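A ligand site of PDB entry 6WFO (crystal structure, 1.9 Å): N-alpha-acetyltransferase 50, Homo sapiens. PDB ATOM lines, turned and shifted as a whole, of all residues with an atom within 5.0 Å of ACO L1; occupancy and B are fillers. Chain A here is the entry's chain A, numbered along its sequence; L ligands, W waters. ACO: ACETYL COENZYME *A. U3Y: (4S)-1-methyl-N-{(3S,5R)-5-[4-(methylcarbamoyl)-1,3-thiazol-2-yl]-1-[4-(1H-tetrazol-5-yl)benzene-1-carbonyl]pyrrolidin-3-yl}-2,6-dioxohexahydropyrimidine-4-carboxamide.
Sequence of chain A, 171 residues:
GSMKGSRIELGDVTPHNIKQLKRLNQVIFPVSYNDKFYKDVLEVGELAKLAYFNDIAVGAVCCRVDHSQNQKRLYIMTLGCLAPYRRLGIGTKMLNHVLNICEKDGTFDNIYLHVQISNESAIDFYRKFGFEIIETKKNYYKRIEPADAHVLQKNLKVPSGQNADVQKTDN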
ATOM      1  N   ILE A  28      31.967   8.355   9.069  1.00  0.00           N
ATOM      2  CA  ILE A  28      31.021   9.028   9.953  1.00  0.00           C
ATOM      3  C   ILE A  28      29.934   9.785   9.201  1.00  0.00           C
ATOM      4  O   ILE A  28      28.793   9.770   9.661  1.00  0.00           O
ATOM      5  CB  ILE A  28      31.769   9.937  11.004  1.00  0.00           C
ATOM      6  CG1 ILE A  28      32.599   9.071  11.989  1.00  0.00           C
ATOM      7  CG2 ILE A  28      30.808  10.892  11.779  1.00  0.00           C
ATOM      8  CD1 ILE A  28      33.808   9.735  12.560  1.00  0.00           C
ATOM      9  N   PHE A  29      30.287  10.464   8.101  1.00  0.00           N
ATOM     10  CA  PHE A  29      29.322  11.298   7.410  1.00  0.00           C
ATOM     11  C   PHE A  29      28.683  10.626   6.183  1.00  0.00           C
ATOM     12  O   PHE A  29      29.364   9.847   5.492  1.00  0.00           O
ATOM     13  CB  PHE A  29      29.949  12.666   7.087  1.00  0.00           C
ATOM     14  CG  PHE A  29      30.389  13.382   8.349  1.00  0.00           C
ATOM     15  CD1 PHE A  29      29.453  13.933   9.219  1.00  0.00           C
ATOM     16  CD2 PHE A  29      31.743  13.411   8.715  1.00  0.00           C
ATOM     17  CE1 PHE A  29      29.858  14.545  10.411  1.00  0.00           C
ATOM     18  CE2 PHE A  29      32.137  14.032   9.907  1.00  0.00           C
ATOM     19  CZ  PHE A  29      31.196  14.615  10.722  1.00  0.00           C
ATOM     20  N   ILE A  76      31.141  25.450  11.277  1.00  0.00           N
ATOM     21  CA  ILE A  76      31.508  24.073  11.564  1.00  0.00           C
ATOM     22  C   ILE A  76      31.052  23.216  10.408  1.00  0.00           C
ATOM     23  O   ILE A  76      29.848  23.046  10.193  1.00  0.00           O
ATOM     24  CB  ILE A  76      31.029  23.518  12.940  1.00  0.00           C
ATOM     25  CG1 ILE A  76      31.443  24.445  14.123  1.00  0.00           C
ATOM     26  CG2 ILE A  76      31.518  22.060  13.167  1.00  0.00           C
ATOM     27  CD1 ILE A  76      30.695  24.126  15.426  1.00  0.00           C
ATOM     28  N   MET A  77      32.020  22.637   9.680  1.00  0.00           N
ATOM     29  CA  MET A  77      31.739  21.817   8.496  1.00  0.00           C
ATOM     30  C   MET A  77      31.421  20.391   8.835  1.00  0.00           C
ATOM     31  O   MET A  77      30.477  19.824   8.319  1.00  0.00           O
ATOM     32  CB  MET A  77      32.929  21.920   7.544  1.00  0.00           C
ATOM     33  CG  MET A  77      33.304  23.353   7.303  1.00  0.00           C
ATOM     34  SD  MET A  77      34.579  23.538   6.072  1.00  0.00           S
ATOM     35  CE  MET A  77      33.651  23.019   4.540  1.00  0.00           C
ATOM     36  N   THR A  78      32.285  19.782   9.634  1.00  0.00           N
ATOM     37  CA  THR A  78      32.188  18.405  10.095  1.00  0.00           C
ATOM     38  C   THR A  78      32.638  18.391  11.535  1.00  0.00           C
ATOM     39  O   THR A  78      33.593  19.073  11.891  1.00  0.00           O
ATOM     40  CB  THR A  78      33.115  17.481   9.253  1.00  0.00           C
ATOM     41  OG1 THR A  78      34.444  18.025   9.253  1.00  0.00           O
ATOM     42  CG2 THR A  78      32.618  17.258   7.827  1.00  0.00           C
ATOM     43  N   LEU A  79      31.932  17.636  12.357  1.00  0.00           N
ATOM     44  CA  LEU A  79      32.209  17.379  13.760  1.00  0.00           C
ATOM     45  C   LEU A  79      31.567  16.030  14.056  1.00  0.00           C
ATOM     46  O   LEU A  79      30.370  15.861  13.922  1.00  0.00           O
ATOM     47  CB  LEU A  79      31.655  18.495  14.691  1.00  0.00           C
ATOM     48  CG  LEU A  79      32.105  18.520  16.197  1.00  0.00           C
ATOM     49  CD1 LEU A  79      32.064  19.949  16.742  1.00  0.00           C
ATOM     50  CD2 LEU A  79      31.225  17.579  17.107  1.00  0.00           C
ATOM     51  N   GLY A  80      32.367  15.043  14.420  1.00  0.00           N
ATOM     52  CA  GLY A  80      31.774  13.764  14.720  1.00  0.00           C
ATOM     53  C   GLY A  80      32.761  12.760  15.220  1.00  0.00           C
ATOM     54  O   GLY A  80      33.959  13.011  15.180  1.00  0.00           O
ATOM     55  N   CYS A  81      32.252  11.614  15.690  1.00  0.00           N
ATOM     56  CA  CYS A  81      33.096  10.549  16.164  1.00  0.00           C
ATOM     57  C   CYS A  81      32.450   9.207  15.894  1.00  0.00           C
ATOM     58  O   CYS A  81      31.232   9.156  15.646  1.00  0.00           O
ATOM     59  CB  CYS A  81      33.566  10.760  17.624  1.00  0.00           C
ATOM     60  SG  CYS A  81      32.575   9.964  18.922  1.00  0.00           S
ATOM     61  N   TYR A  85      32.099   5.009  20.166  1.00  0.00           N
ATOM     62  CA  TYR A  85      32.764   5.940  21.092  1.00  0.00           C
ATOM     63  C   TYR A  85      31.889   7.144  21.460  1.00  0.00           C
ATOM     64  O   TYR A  85      32.326   8.023  22.200  1.00  0.00           O
ATOM     65  CB  TYR A  85      34.100   6.406  20.485  1.00  0.00           C
ATOM     66  CG  TYR A  85      35.073   5.258  20.351  1.00  0.00           C
ATOM     67  CD1 TYR A  85      35.779   4.778  21.456  1.00  0.00           C
ATOM     68  CD2 TYR A  85      35.220   4.585  19.142  1.00  0.00           C
ATOM     69  CE1 TYR A  85      36.638   3.690  21.344  1.00  0.00           C
ATOM     70  CE2 TYR A  85      36.079   3.498  19.013  1.00  0.00           C
ATOM     71  CZ  TYR A  85      36.792   3.060  20.120  1.00  0.00           C
ATOM     72  OH  TYR A  85      37.622   1.969  20.014  1.00  0.00           O
ATOM     73  N   ARG A  86      30.649   7.180  20.929  1.00  0.00           N
ATOM     74  CA  ARG A  86      29.719   8.270  21.181  1.00  0.00           C
ATOM     75  C   ARG A  86      29.242   8.229  22.619  1.00  0.00           C
ATOM     76  O   ARG A  86      29.314   7.180  23.238  1.00  0.00           O
ATOM     77  CB  ARG A  86      28.559   8.229  20.187  1.00  0.00           C
ATOM     78  CG  ARG A  86      29.000   8.724  18.830  1.00  0.00           C
ATOM     79  CD  ARG A  86      27.941   8.476  17.769  1.00  0.00           C
ATOM     80  NE  ARG A  86      28.555   8.653  16.459  1.00  0.00           N
ATOM     81  CZ  ARG A  86      27.991   8.301  15.309  1.00  0.00           C
ATOM     82  NH1 ARG A  86      26.761   7.814  15.288  1.00  0.00           N
ATOM     83  NH2 ARG A  86      28.649   8.474  14.166  1.00  0.00           N
ATOM     84  N   ARG A  87      28.800   9.380  23.146  1.00  0.00           N
ATOM     85  CA  ARG A  87      28.299   9.561  24.525  1.00  0.00           C
ATOM     86  C   ARG A  87      29.370   9.299  25.558  1.00  0.00           C
ATOM     87  O   ARG A  87      29.085   8.739  26.630  1.00  0.00           O
ATOM     88  CB  ARG A  87      27.017   8.746  24.841  1.00  0.00           C
ATOM     89  CG  ARG A  87      25.823   9.068  23.970  1.00  0.00           C
ATOM     90  CD  ARG A  87      25.358  10.513  24.117  1.00  0.00           C
ATOM     91  NE  ARG A  87      24.743  10.819  25.412  1.00  0.00           N
ATOM     92  CZ  ARG A  87      23.448  10.676  25.681  1.00  0.00           C
ATOM     93  NH1 ARG A  87      22.623  10.187  24.763  1.00  0.00           N
ATOM     94  NH2 ARG A  87      22.962  11.025  26.873  1.00  0.00           N
ATOM     95  N   LEU A  88      30.629   9.716  25.244  1.00  0.00           N
ATOM     96  CA  LEU A  88      31.769   9.594  26.147  1.00  0.00           C
ATOM     97  C   LEU A  88      32.405  10.962  26.367  1.00  0.00           C
ATOM     98  O   LEU A  88      33.385  11.028  27.111  1.00  0.00           O
ATOM     99  CB  LEU A  88      32.830   8.586  25.621  1.00  0.00           C
ATOM    100  CG  LEU A  88      32.446   7.081  25.655  1.00  0.00           C
ATOM    101  CD1 LEU A  88      33.552   6.216  25.017  1.00  0.00           C
ATOM    102  CD2 LEU A  88      32.116   6.592  27.086  1.00  0.00           C
ATOM    103  N   GLY A  89      31.892  12.000  25.707  1.00  0.00           N
ATOM    104  CA  GLY A  89      32.397  13.359  25.848  1.00  0.00           C
ATOM    105  C   GLY A  89      33.276  13.847  24.711  1.00  0.00           C
ATOM    106  O   GLY A  89      33.759  14.985  24.762  1.00  0.00           O
ATOM    107  N   ILE A  90      33.464  13.022  23.647  1.00  0.00           N
ATOM    108  CA  ILE A  90      34.351  13.350  22.523  1.00  0.00           C
ATOM    109  C   ILE A  90      33.808  14.530  21.734  1.00  0.00           C
ATOM    110  O   ILE A  90      34.575  15.430  21.424  1.00  0.00           O
ATOM    111  CB  ILE A  90      34.722  12.118  21.644  1.00  0.00           C
ATOM    112  CG1 ILE A  90      35.594  11.128  22.442  1.00  0.00           C
ATOM    113  CG2 ILE A  90      35.436  12.529  20.331  1.00  0.00           C
ATOM    114  CD1 ILE A  90      35.433   9.726  22.091  1.00  0.00           C
ATOM    115  N   GLY A  91      32.502  14.532  21.450  1.00  0.00           N
ATOM    116  CA  GLY A  91      31.802  15.623  20.773  1.00  0.00           C
ATOM    117  C   GLY A  91      31.964  16.911  21.556  1.00  0.00           C
ATOM    118  O   GLY A  91      32.409  17.909  20.973  1.00  0.00           O
ATOM    119  N   THR A  92      31.648  16.884  22.906  1.00  0.00           N
ATOM    120  CA  THR A  92      31.826  18.022  23.852  1.00  0.00           C
ATOM    121  C   THR A  92      33.264  18.601  23.813  1.00  0.00           C
ATOM    122  O   THR A  92      33.415  19.819  23.799  1.00  0.00           O
ATOM    123  CB  THR A  92      31.475  17.628  25.324  1.00  0.00           C
ATOM    124  OG1 THR A  92      30.111  17.273  25.377  1.00  0.00           O
ATOM    125  CG2 THR A  92      31.713  18.746  26.320  1.00  0.00           C
ATOM    126  N   LEU A 113      26.305  26.011  11.633  1.00  0.00           N
ATOM    127  CA  LEU A 113      26.482  24.726  10.950  1.00  0.00           C
ATOM    128  C   LEU A 113      25.140  24.295  10.338  1.00  0.00           C
ATOM    129  O   LEU A 113      24.102  24.890  10.651  1.00  0.00           O
ATOM    130  CB  LEU A 113      26.946  23.685  12.004  1.00  0.00           C
ATOM    131  CG  LEU A 113      25.999  23.574  13.265  1.00  0.00           C
ATOM    132  CD1 LEU A 113      25.562  22.204  13.470  1.00  0.00           C
ATOM    133  CD2 LEU A 113      26.632  24.061  14.480  1.00  0.00           C
ATOM    134  N   HIS A 114      25.166  23.253   9.499  1.00  0.00           N
ATOM    135  CA  HIS A 114      23.974  22.644   8.920  1.00  0.00           C
ATOM    136  C   HIS A 114      23.855  21.243   9.478  1.00  0.00           C
ATOM    137  O   HIS A 114      24.898  20.578   9.692  1.00  0.00           O
ATOM    138  CB  HIS A 114      24.040  22.615   7.395  1.00  0.00           C
ATOM    139  CG  HIS A 114      23.913  23.968   6.768  1.00  0.00           C
ATOM    140  ND1 HIS A 114      25.027  24.730   6.485  1.00  0.00           N
ATOM    141  CD2 HIS A 114      22.801  24.641   6.387  1.00  0.00           C
ATOM    142  CE1 HIS A 114      24.576  25.858   5.940  1.00  0.00           C
ATOM    143  NE2 HIS A 114      23.236  25.846   5.847  1.00  0.00           N
ATOM    144  N   VAL A 115      22.622  20.795   9.760  1.00  0.00           N
ATOM    145  CA  VAL A 115      22.344  19.456  10.301  1.00  0.00           C
ATOM    146  C   VAL A 115      21.190  18.914   9.488  1.00  0.00           C
ATOM    147  O   VAL A 115      20.122  19.517   9.524  1.00  0.00           O
ATOM    148  CB  VAL A 115      21.947  19.461  11.816  1.00  0.00           C
ATOM    149  CG1 VAL A 115      21.791  18.038  12.350  1.00  0.00           C
ATOM    150  CG2 VAL A 115      22.920  20.259  12.683  1.00  0.00           C
ATOM    151  N   ASN A 119      18.714  14.018  11.803  1.00  0.00           N
ATOM    152  CA  ASN A 119      19.737  13.821  12.836  1.00  0.00           C
ATOM    153  C   ASN A 119      19.336  14.439  14.201  1.00  0.00           C
ATOM    154  O   ASN A 119      19.799  15.502  14.583  1.00  0.00           O
ATOM    155  CB  ASN A 119      21.071  14.367  12.327  1.00  0.00           C
ATOM    156  CG  ASN A 119      22.289  13.768  12.972  1.00  0.00           C
ATOM    157  OD1 ASN A 119      22.261  13.229  14.071  1.00  0.00           O
ATOM    158  ND2 ASN A 119      23.390  13.876  12.276  1.00  0.00           N
ATOM    159  N   SER A 121      19.872  13.328  17.321  1.00  0.00           N
ATOM    160  CA  SER A 121      21.024  13.255  18.221  1.00  0.00           C
ATOM    161  C   SER A 121      21.929  14.523  18.072  1.00  0.00           C
ATOM    162  O   SER A 121      22.295  15.124  19.084  1.00  0.00           O
ATOM    163  CB  SER A 121      21.796  11.961  17.940  1.00  0.00           C
ATOM    164  OG  SER A 121      23.197  12.051  18.130  1.00  0.00           O
ATOM    165  N   ALA A 122      22.270  14.919  16.832  1.00  0.00           N
ATOM    166  CA  ALA A 122      23.104  16.119  16.587  1.00  0.00           C
ATOM    167  C   ALA A 122      22.363  17.384  17.010  1.00  0.00           C
ATOM    168  O   ALA A 122      22.978  18.197  17.651  1.00  0.00           O
ATOM    169  CB  ALA A 122      23.547  16.211  15.123  1.00  0.00           C
ATOM    170  N   ASP A 124      19.994  17.736  19.373  1.00  0.00           N
ATOM    171  CA  ASP A 124      20.001  17.636  20.825  1.00  0.00           C
ATOM    172  C   ASP A 124      21.378  18.036  21.376  1.00  0.00           C
ATOM    173  O   ASP A 124      21.451  18.811  22.329  1.00  0.00           O
ATOM    174  CB  ASP A 124      19.713  16.185  21.237  1.00  0.00           C
ATOM    175  CG  ASP A 124      18.589  15.969  22.221  1.00  0.00           C
ATOM    176  OD1 ASP A 124      18.224  16.931  22.937  1.00  0.00           O
ATOM    177  OD2 ASP A 124      18.102  14.837  22.321  1.00  0.00           O
ATOM    178  N   PHE A 125      22.459  17.495  20.783  1.00  0.00           N
ATOM    179  CA  PHE A 125      23.844  17.799  21.131  1.00  0.00           C
ATOM    180  C   PHE A 125      24.107  19.305  21.042  1.00  0.00           C
ATOM    181  O   PHE A 125      24.496  19.926  22.026  1.00  0.00           O
ATOM    182  CB  PHE A 125      24.836  17.005  20.233  1.00  0.00           C
ATOM    183  CG  PHE A 125      26.281  17.397  20.396  1.00  0.00           C
ATOM    184  CD1 PHE A 125      27.004  16.971  21.510  1.00  0.00           C
ATOM    185  CD2 PHE A 125      26.899  18.230  19.476  1.00  0.00           C
ATOM    186  CE1 PHE A 125      28.334  17.367  21.680  1.00  0.00           C
ATOM    187  CE2 PHE A 125      28.228  18.647  19.653  1.00  0.00           C
ATOM    188  CZ  PHE A 125      28.930  18.218  20.762  1.00  0.00           C
ATOM    189  N   TYR A 126      23.828  19.898  19.886  1.00  0.00           N
ATOM    190  CA  TYR A 126      24.135  21.310  19.703  1.00  0.00           C
ATOM    191  C   TYR A 126      23.290  22.277  20.547  1.00  0.00           C
ATOM    192  O   TYR A 126      23.814  23.297  21.006  1.00  0.00           O
ATOM    193  CB  TYR A 126      24.074  21.656  18.245  1.00  0.00           C
ATOM    194  CG  TYR A 126      25.289  21.204  17.482  1.00  0.00           C
ATOM    195  CD1 TYR A 126      26.500  21.896  17.592  1.00  0.00           C
ATOM    196  CD2 TYR A 126      25.230  20.151  16.586  1.00  0.00           C
ATOM    197  CE1 TYR A 126      27.632  21.505  16.880  1.00  0.00           C
ATOM    198  CE2 TYR A 126      26.357  19.732  15.872  1.00  0.00           C
ATOM    199  CZ  TYR A 126      27.544  20.427  16.001  1.00  0.00           C
ATOM    200  OH  TYR A 126      28.615  20.078  15.229  1.00  0.00           O
ATOM    201  N   LYS A 128      22.321  21.831  23.517  1.00  0.00           N
ATOM    202  CA  LYS A 128      22.864  21.793  24.867  1.00  0.00           C
ATOM    203  C   LYS A 128      23.931  22.886  25.040  1.00  0.00           C
ATOM    204  O   LYS A 128      24.114  23.367  26.139  1.00  0.00           O
ATOM    205  CB  LYS A 128      23.461  20.406  25.155  1.00  0.00           C
ATOM    206  CG  LYS A 128      23.777  20.147  26.627  1.00  0.00           C
ATOM    207  CD  LYS A 128      24.900  19.112  26.793  1.00  0.00           C
ATOM    208  CE  LYS A 128      25.254  18.813  28.233  1.00  0.00           C
ATOM    209  NZ  LYS A 128      24.222  17.962  28.908  1.00  0.00           N
ATOM    210  N   PHE A 129      24.568  23.332  23.938  1.00  0.00           N
ATOM    211  CA  PHE A 129      25.624  24.357  23.962  1.00  0.00           C
ATOM    212  C   PHE A 129      25.118  25.745  23.649  1.00  0.00           C
ATOM    213  O   PHE A 129      25.929  26.660  23.531  1.00  0.00           O
ATOM    214  CB  PHE A 129      26.804  23.964  23.036  1.00  0.00           C
ATOM    215  CG  PHE A 129      27.541  22.743  23.530  1.00  0.00           C
ATOM    216  CD1 PHE A 129      27.062  21.459  23.267  1.00  0.00           C
ATOM    217  CD2 PHE A 129      28.756  22.866  24.216  1.00  0.00           C
ATOM    218  CE1 PHE A 129      27.723  20.336  23.758  1.00  0.00           C
ATOM    219  CE2 PHE A 129      29.439  21.728  24.671  1.00  0.00           C
ATOM    220  CZ  PHE A 129      28.919  20.471  24.439  1.00  0.00           C
HETATM  221  N1A ACO L   1      20.699  11.629  22.389  1.00  0.00           N
HETATM  222  C2A ACO L   1      20.449  12.644  23.222  1.00  0.00           C
HETATM  223  N3A ACO L   1      21.281  13.608  23.645  1.00  0.00           N
HETATM  224  C4A ACO L   1      22.495  13.473  23.088  1.00  0.00           C
HETATM  225  C5A ACO L   1      22.891  12.496  22.197  1.00  0.00           C
HETATM  226  C6A ACO L   1      21.939  11.526  21.839  1.00  0.00           C
HETATM  227  N6A ACO L   1      22.187  10.496  21.022  1.00  0.00           N
HETATM  228  N7A ACO L   1      24.215  12.683  21.827  1.00  0.00           N
HETATM  229  C8A ACO L   1      24.582  13.751  22.494  1.00  0.00           C
HETATM  230  N9A ACO L   1      23.608  14.262  23.298  1.00  0.00           N
HETATM  231  C1B ACO L   1      23.746  15.348  24.270  1.00  0.00           C
HETATM  232  C2B ACO L   1      23.666  14.873  25.733  1.00  0.00           C
HETATM  233  O2B ACO L   1      23.005  15.796  26.583  1.00  0.00           O
HETATM  234  C3B ACO L   1      25.154  14.689  26.037  1.00  0.00           C
HETATM  235  O3B ACO L   1      25.452  14.738  27.448  1.00  0.00           O
HETATM  236  P3B ACO L   1      25.427  13.379  28.331  1.00  0.00           P
HETATM  237  O7A ACO L   1      26.179  13.650  29.595  1.00  0.00           O
HETATM  238  O8A ACO L   1      23.901  13.070  28.545  1.00  0.00           O
HETATM  239  O9A ACO L   1      26.048  12.264  27.446  1.00  0.00           O
HETATM  240  C4B ACO L   1      25.793  15.858  25.312  1.00  0.00           C
HETATM  241  O4B ACO L   1      25.015  15.956  24.091  1.00  0.00           O
HETATM  242  C5B ACO L   1      27.259  15.733  24.984  1.00  0.00           C
HETATM  243  O5B ACO L   1      27.500  14.497  24.257  1.00  0.00           O
HETATM  244  P1A ACO L   1      28.957  13.915  23.910  1.00  0.00           P
HETATM  245  O1A ACO L   1      29.279  12.722  24.678  1.00  0.00           O
HETATM  246  O2A ACO L   1      30.052  14.936  24.003  1.00  0.00           O
HETATM  247  O3A ACO L   1      28.698  13.567  22.369  1.00  0.00           O
HETATM  248  P2A ACO L   1      29.323  12.692  21.192  1.00  0.00           P
HETATM  249  O4A ACO L   1      30.744  12.385  21.466  1.00  0.00           O
HETATM  250  O5A ACO L   1      28.536  11.417  21.148  1.00  0.00           O
HETATM  251  O6A ACO L   1      29.141  13.689  19.981  1.00  0.00           O
HETATM  252  CBP ACO L   1      27.758  13.811  17.890  1.00  0.00           C
HETATM  253  CCP ACO L   1      27.826  13.904  19.417  1.00  0.00           C
HETATM  254  CDP ACO L   1      28.931  14.605  17.278  1.00  0.00           C
HETATM  255  CEP ACO L   1      26.446  14.436  17.410  1.00  0.00           C
HETATM  256  CAP ACO L   1      27.878  12.308  17.512  1.00  0.00           C
HETATM  257  OAP ACO L   1      26.688  11.604  17.869  1.00  0.00           O
HETATM  258  C9P ACO L   1      28.249  11.949  16.089  1.00  0.00           C
HETATM  259  O9P ACO L   1      29.419  11.683  15.807  1.00  0.00           O
HETATM  260  N8P ACO L   1      27.247  11.846  15.205  1.00  0.00           N
HETATM  261  C7P ACO L   1      27.453  11.565  13.795  1.00  0.00           C
HETATM  262  C6P ACO L   1      27.923  12.784  13.047  1.00  0.00           C
HETATM  263  C5P ACO L   1      27.071  13.987  13.380  1.00  0.00           C
HETATM  264  O5P ACO L   1      25.849  13.895  13.448  1.00  0.00           O
HETATM  265  N4P ACO L   1      27.716  15.132  13.574  1.00  0.00           N
HETATM  266  C3P ACO L   1      27.041  16.417  13.511  1.00  0.00           C
HETATM  267  C2P ACO L   1      26.568  16.692  12.094  1.00  0.00           C
HETATM  268  S1P ACO L   1      26.589  18.462  11.863  1.00  0.00           S
HETATM  269  C   ACO L   1      28.313  18.748  11.621  1.00  0.00           C
HETATM  270  O   ACO L   1      29.099  17.854  11.460  1.00  0.00           O
HETATM  271  CH3 ACO L   1      28.649  20.202  11.481  1.00  0.00           C
HETATM  272  C19 U3Y L   2      26.416  18.395   0.224  1.00  0.00           C
HETATM  273  C21 U3Y L   2      28.308  16.900  -0.101  1.00  0.00           C
HETATM  274  C18 U3Y L   2      27.263  19.354   0.802  1.00  0.00           C
HETATM  275  C22 U3Y L   2      29.164  17.858   0.482  1.00  0.00           C
HETATM  276  C7  U3Y L   2      28.589  25.224   2.634  1.00  0.00           C
HETATM  277  C20 U3Y L   2      26.943  17.175  -0.233  1.00  0.00           C
HETATM  278  C17 U3Y L   2      28.626  19.066   0.933  1.00  0.00           C
HETATM  279  C6  U3Y L   2      29.805  25.330   3.261  1.00  0.00           C
HETATM  280  C23 U3Y L   2      26.033  16.163  -0.826  1.00  0.00           C
HETATM  281  C5  U3Y L   2      29.708  23.112   3.163  1.00  0.00           C
HETATM  282  C13 U3Y L   2      27.547  16.332   7.197  1.00  0.00           C
HETATM  283  C14 U3Y L   2      25.423  17.138   8.244  1.00  0.00           C
HETATM  284  C16 U3Y L   2      29.532  20.050   1.524  1.00  0.00           C
HETATM  285  C8  U3Y L   2      30.400  26.602   3.637  1.00  0.00           C
HETATM  286  C10 U3Y L   2      27.239  19.438   6.681  1.00  0.00           C
HETATM  287  C12 U3Y L   2      28.209  17.499   7.930  1.00  0.00           C
HETATM  288  C4  U3Y L   2      29.942  21.321   4.883  1.00  0.00           C
HETATM  289  C2  U3Y L   2      28.388  19.907   3.798  1.00  0.00           C
HETATM  290  C1  U3Y L   2      30.050  21.642   3.386  1.00  0.00           C
HETATM  291  C11 U3Y L   2      27.331  18.736   8.006  1.00  0.00           C
HETATM  292  C3  U3Y L   2      28.516  20.790   5.046  1.00  0.00           C
HETATM  293  C15 U3Y L   2      25.351  15.299   6.626  1.00  0.00           C
HETATM  294  N10 U3Y L   2      24.715  16.356  -1.033  1.00  0.00           N
HETATM  295  N2  U3Y L   2      30.436  24.131   3.556  1.00  0.00           N
HETATM  296  N7  U3Y L   2      26.421  14.906  -1.145  1.00  0.00           N
HETATM  297  N9  U3Y L   2      24.271  15.165  -1.498  1.00  0.00           N
HETATM  298  N8  U3Y L   2      25.290  14.293  -1.581  1.00  0.00           N
HETATM  299  N6  U3Y L   2      25.990  18.390   8.423  1.00  0.00           N
HETATM  300  N5  U3Y L   2      26.129  16.319   7.325  1.00  0.00           N
HETATM  301  N1  U3Y L   2      29.180  20.604   2.763  1.00  0.00           N
HETATM  302  N4  U3Y L   2      28.382  20.106   6.328  1.00  0.00           N
HETATM  303  O4  U3Y L   2      28.227  15.512   6.602  1.00  0.00           O
HETATM  304  O3  U3Y L   2      24.402  16.781   8.802  1.00  0.00           O
HETATM  305  O5  U3Y L   2      30.530  20.310   0.862  1.00  0.00           O
HETATM  306  O1  U3Y L   2      29.833  27.439   4.342  1.00  0.00           O
HETATM  307  O2  U3Y L   2      26.243  19.416   5.976  1.00  0.00           O
HETATM  308  S1  U3Y L   2      28.253  23.563   2.408  1.00  0.00           S
HETATM  309  O   HOH W   1      25.934  11.040  20.435  1.00  0.00           O
HETATM  310  O   HOH W   2      28.726  12.482  27.407  1.00  0.00           O
HETATM  311  O   HOH W   3      24.681   8.670  20.059  1.00  0.00           O
HETATM  312  O   HOH W   4      32.026  10.576  22.800  1.00  0.00           O
HETATM  313  O   HOH W   5      24.154  11.648  15.209  1.00  0.00           O
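A nitrogen (N6) of U3Y L2 sits close to a sulfur (S1P) of ACO L1 (3.5 Å).
The side-chain amino group (NZ) of Lys 128 sits at hydrogen-bond distance from an oxygen (O2B) of ACO L1.
ND2 of Asn 119 is in hydrogen-bond range of O5P of ACO L1.
The backbone NH of Cys 81 is in hydrogen-bond range of an oxygen (O9P) of ACO L1, 2.8 Å away.
The side-chain hydroxyl (OG) of Ser 121 lies close to a nitrogen (N6A) of ACO L1 (3.4 Å).
O of His 114 is in hydrogen-bond range of N6 of U3Y L2 (2.8 Å).
An oxygen (O2A) of ACO L1 lies within hydrogen-bond range of the side-chain hydroxyl (OG1) of Thr 92, 2.7 Å away.
The backbone NH (N) of Gly 91 is in hydrogen-bond range of an oxygen (O4A) of ACO L1, 2.8 Å away.
The backbone NH (N) of Thr 92 is in hydrogen-bond range of an oxygen (O2A) of ACO L1 (2.7 Å).
The backbone NH (N) of Leu 79 is in hydrogen-bond range of an oxygen (O) of ACO L1, 3.0 Å away.
The backbone carbonyl oxygen of Leu 79 sits at hydrogen-bond distance from a nitrogen (N4P) of ACO L1, 2.8 Å away.
N4 of U3Y L2 sits at hydrogen-bond distance from O of Met 77 (2.9 Å).
The guanidinium group (NE) of Arg 86 is in hydrogen-bond range of an oxygen (O9P) of ACO L1.
An oxygen (O1A) of ACO L1 is in hydrogen-bond range of the backbone NH (N) of Gly 89 (2.9 Å).
The guanidinium group (NH2) of Arg 87 is in salt-bridge range of an oxygen (O8A) of ACO L1.
An oxygen (O5A) of ACO L1 is in hydrogen-bond range of the backbone NH (N) of Arg 87, 2.9 Å away.
An oxygen (O1A) of ACO L1 is in hydrogen-bond range of the backbone NH (N) of Leu 88, at 3.3 Å.
S1P of ACO L1 lies close to O of His 114 (3.5 Å).
CG2 of Ile 28 touches C6P of ACO L1 (3.7 Å).
Phe 29 touches ACO L1 (CE1 to O, 3.6 Å).
Ile 76 touches ACO L1.
Met 77 touches ACO L1.
Thr 78 touches ACO L1 (CA to O, 3.4 Å).
CA of Gly 80 touches O9P of ACO L1 (3.3 Å).
Ile 90 touches ACO L1 (N to O4A, 3.5 Å).
Leu 113 touches ACO L1 (CB to CH3, 3.9 Å).
Ala 122 touches ACO L1.
Asp 124 touches ACO L1 (OD2 to C2A, 3.3 Å).
CD1 of Phe 125 touches O4B of ACO L1 (3.4 Å).
Tyr 126 touches ACO L1 (OH to CH3, 3.8 Å).
Hydrophobic or aromatic side chains that line ACO L1: Ile 28, Phe 29, Ile 76, Leu 79, Ile 90, Leu 113, Ala 122 and Phe 125.
Of the 27 residues printed, 24 come within 4 Å of ACO L1.
The nearest printed residue that does not touch ACO L1 is Val 115 (4.2 Å).
The side-chain amide oxygen (OD1) of Asn 119 lies within hydrogen-bond range of the backbone NH (N) of Ala 122 (3.2 Å).
The guanidinium group (NE) of Arg 86 lies within hydrogen-bond range of the backbone carbonyl oxygen (O) of Cys 81 (2.8 Å).
Water W5 lies within hydrogen-bond range of OD1 of Asn 119 (2.7 Å), N8P of ACO L1 (3.1 Å) and OG of Ser 121 (3.1 Å).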
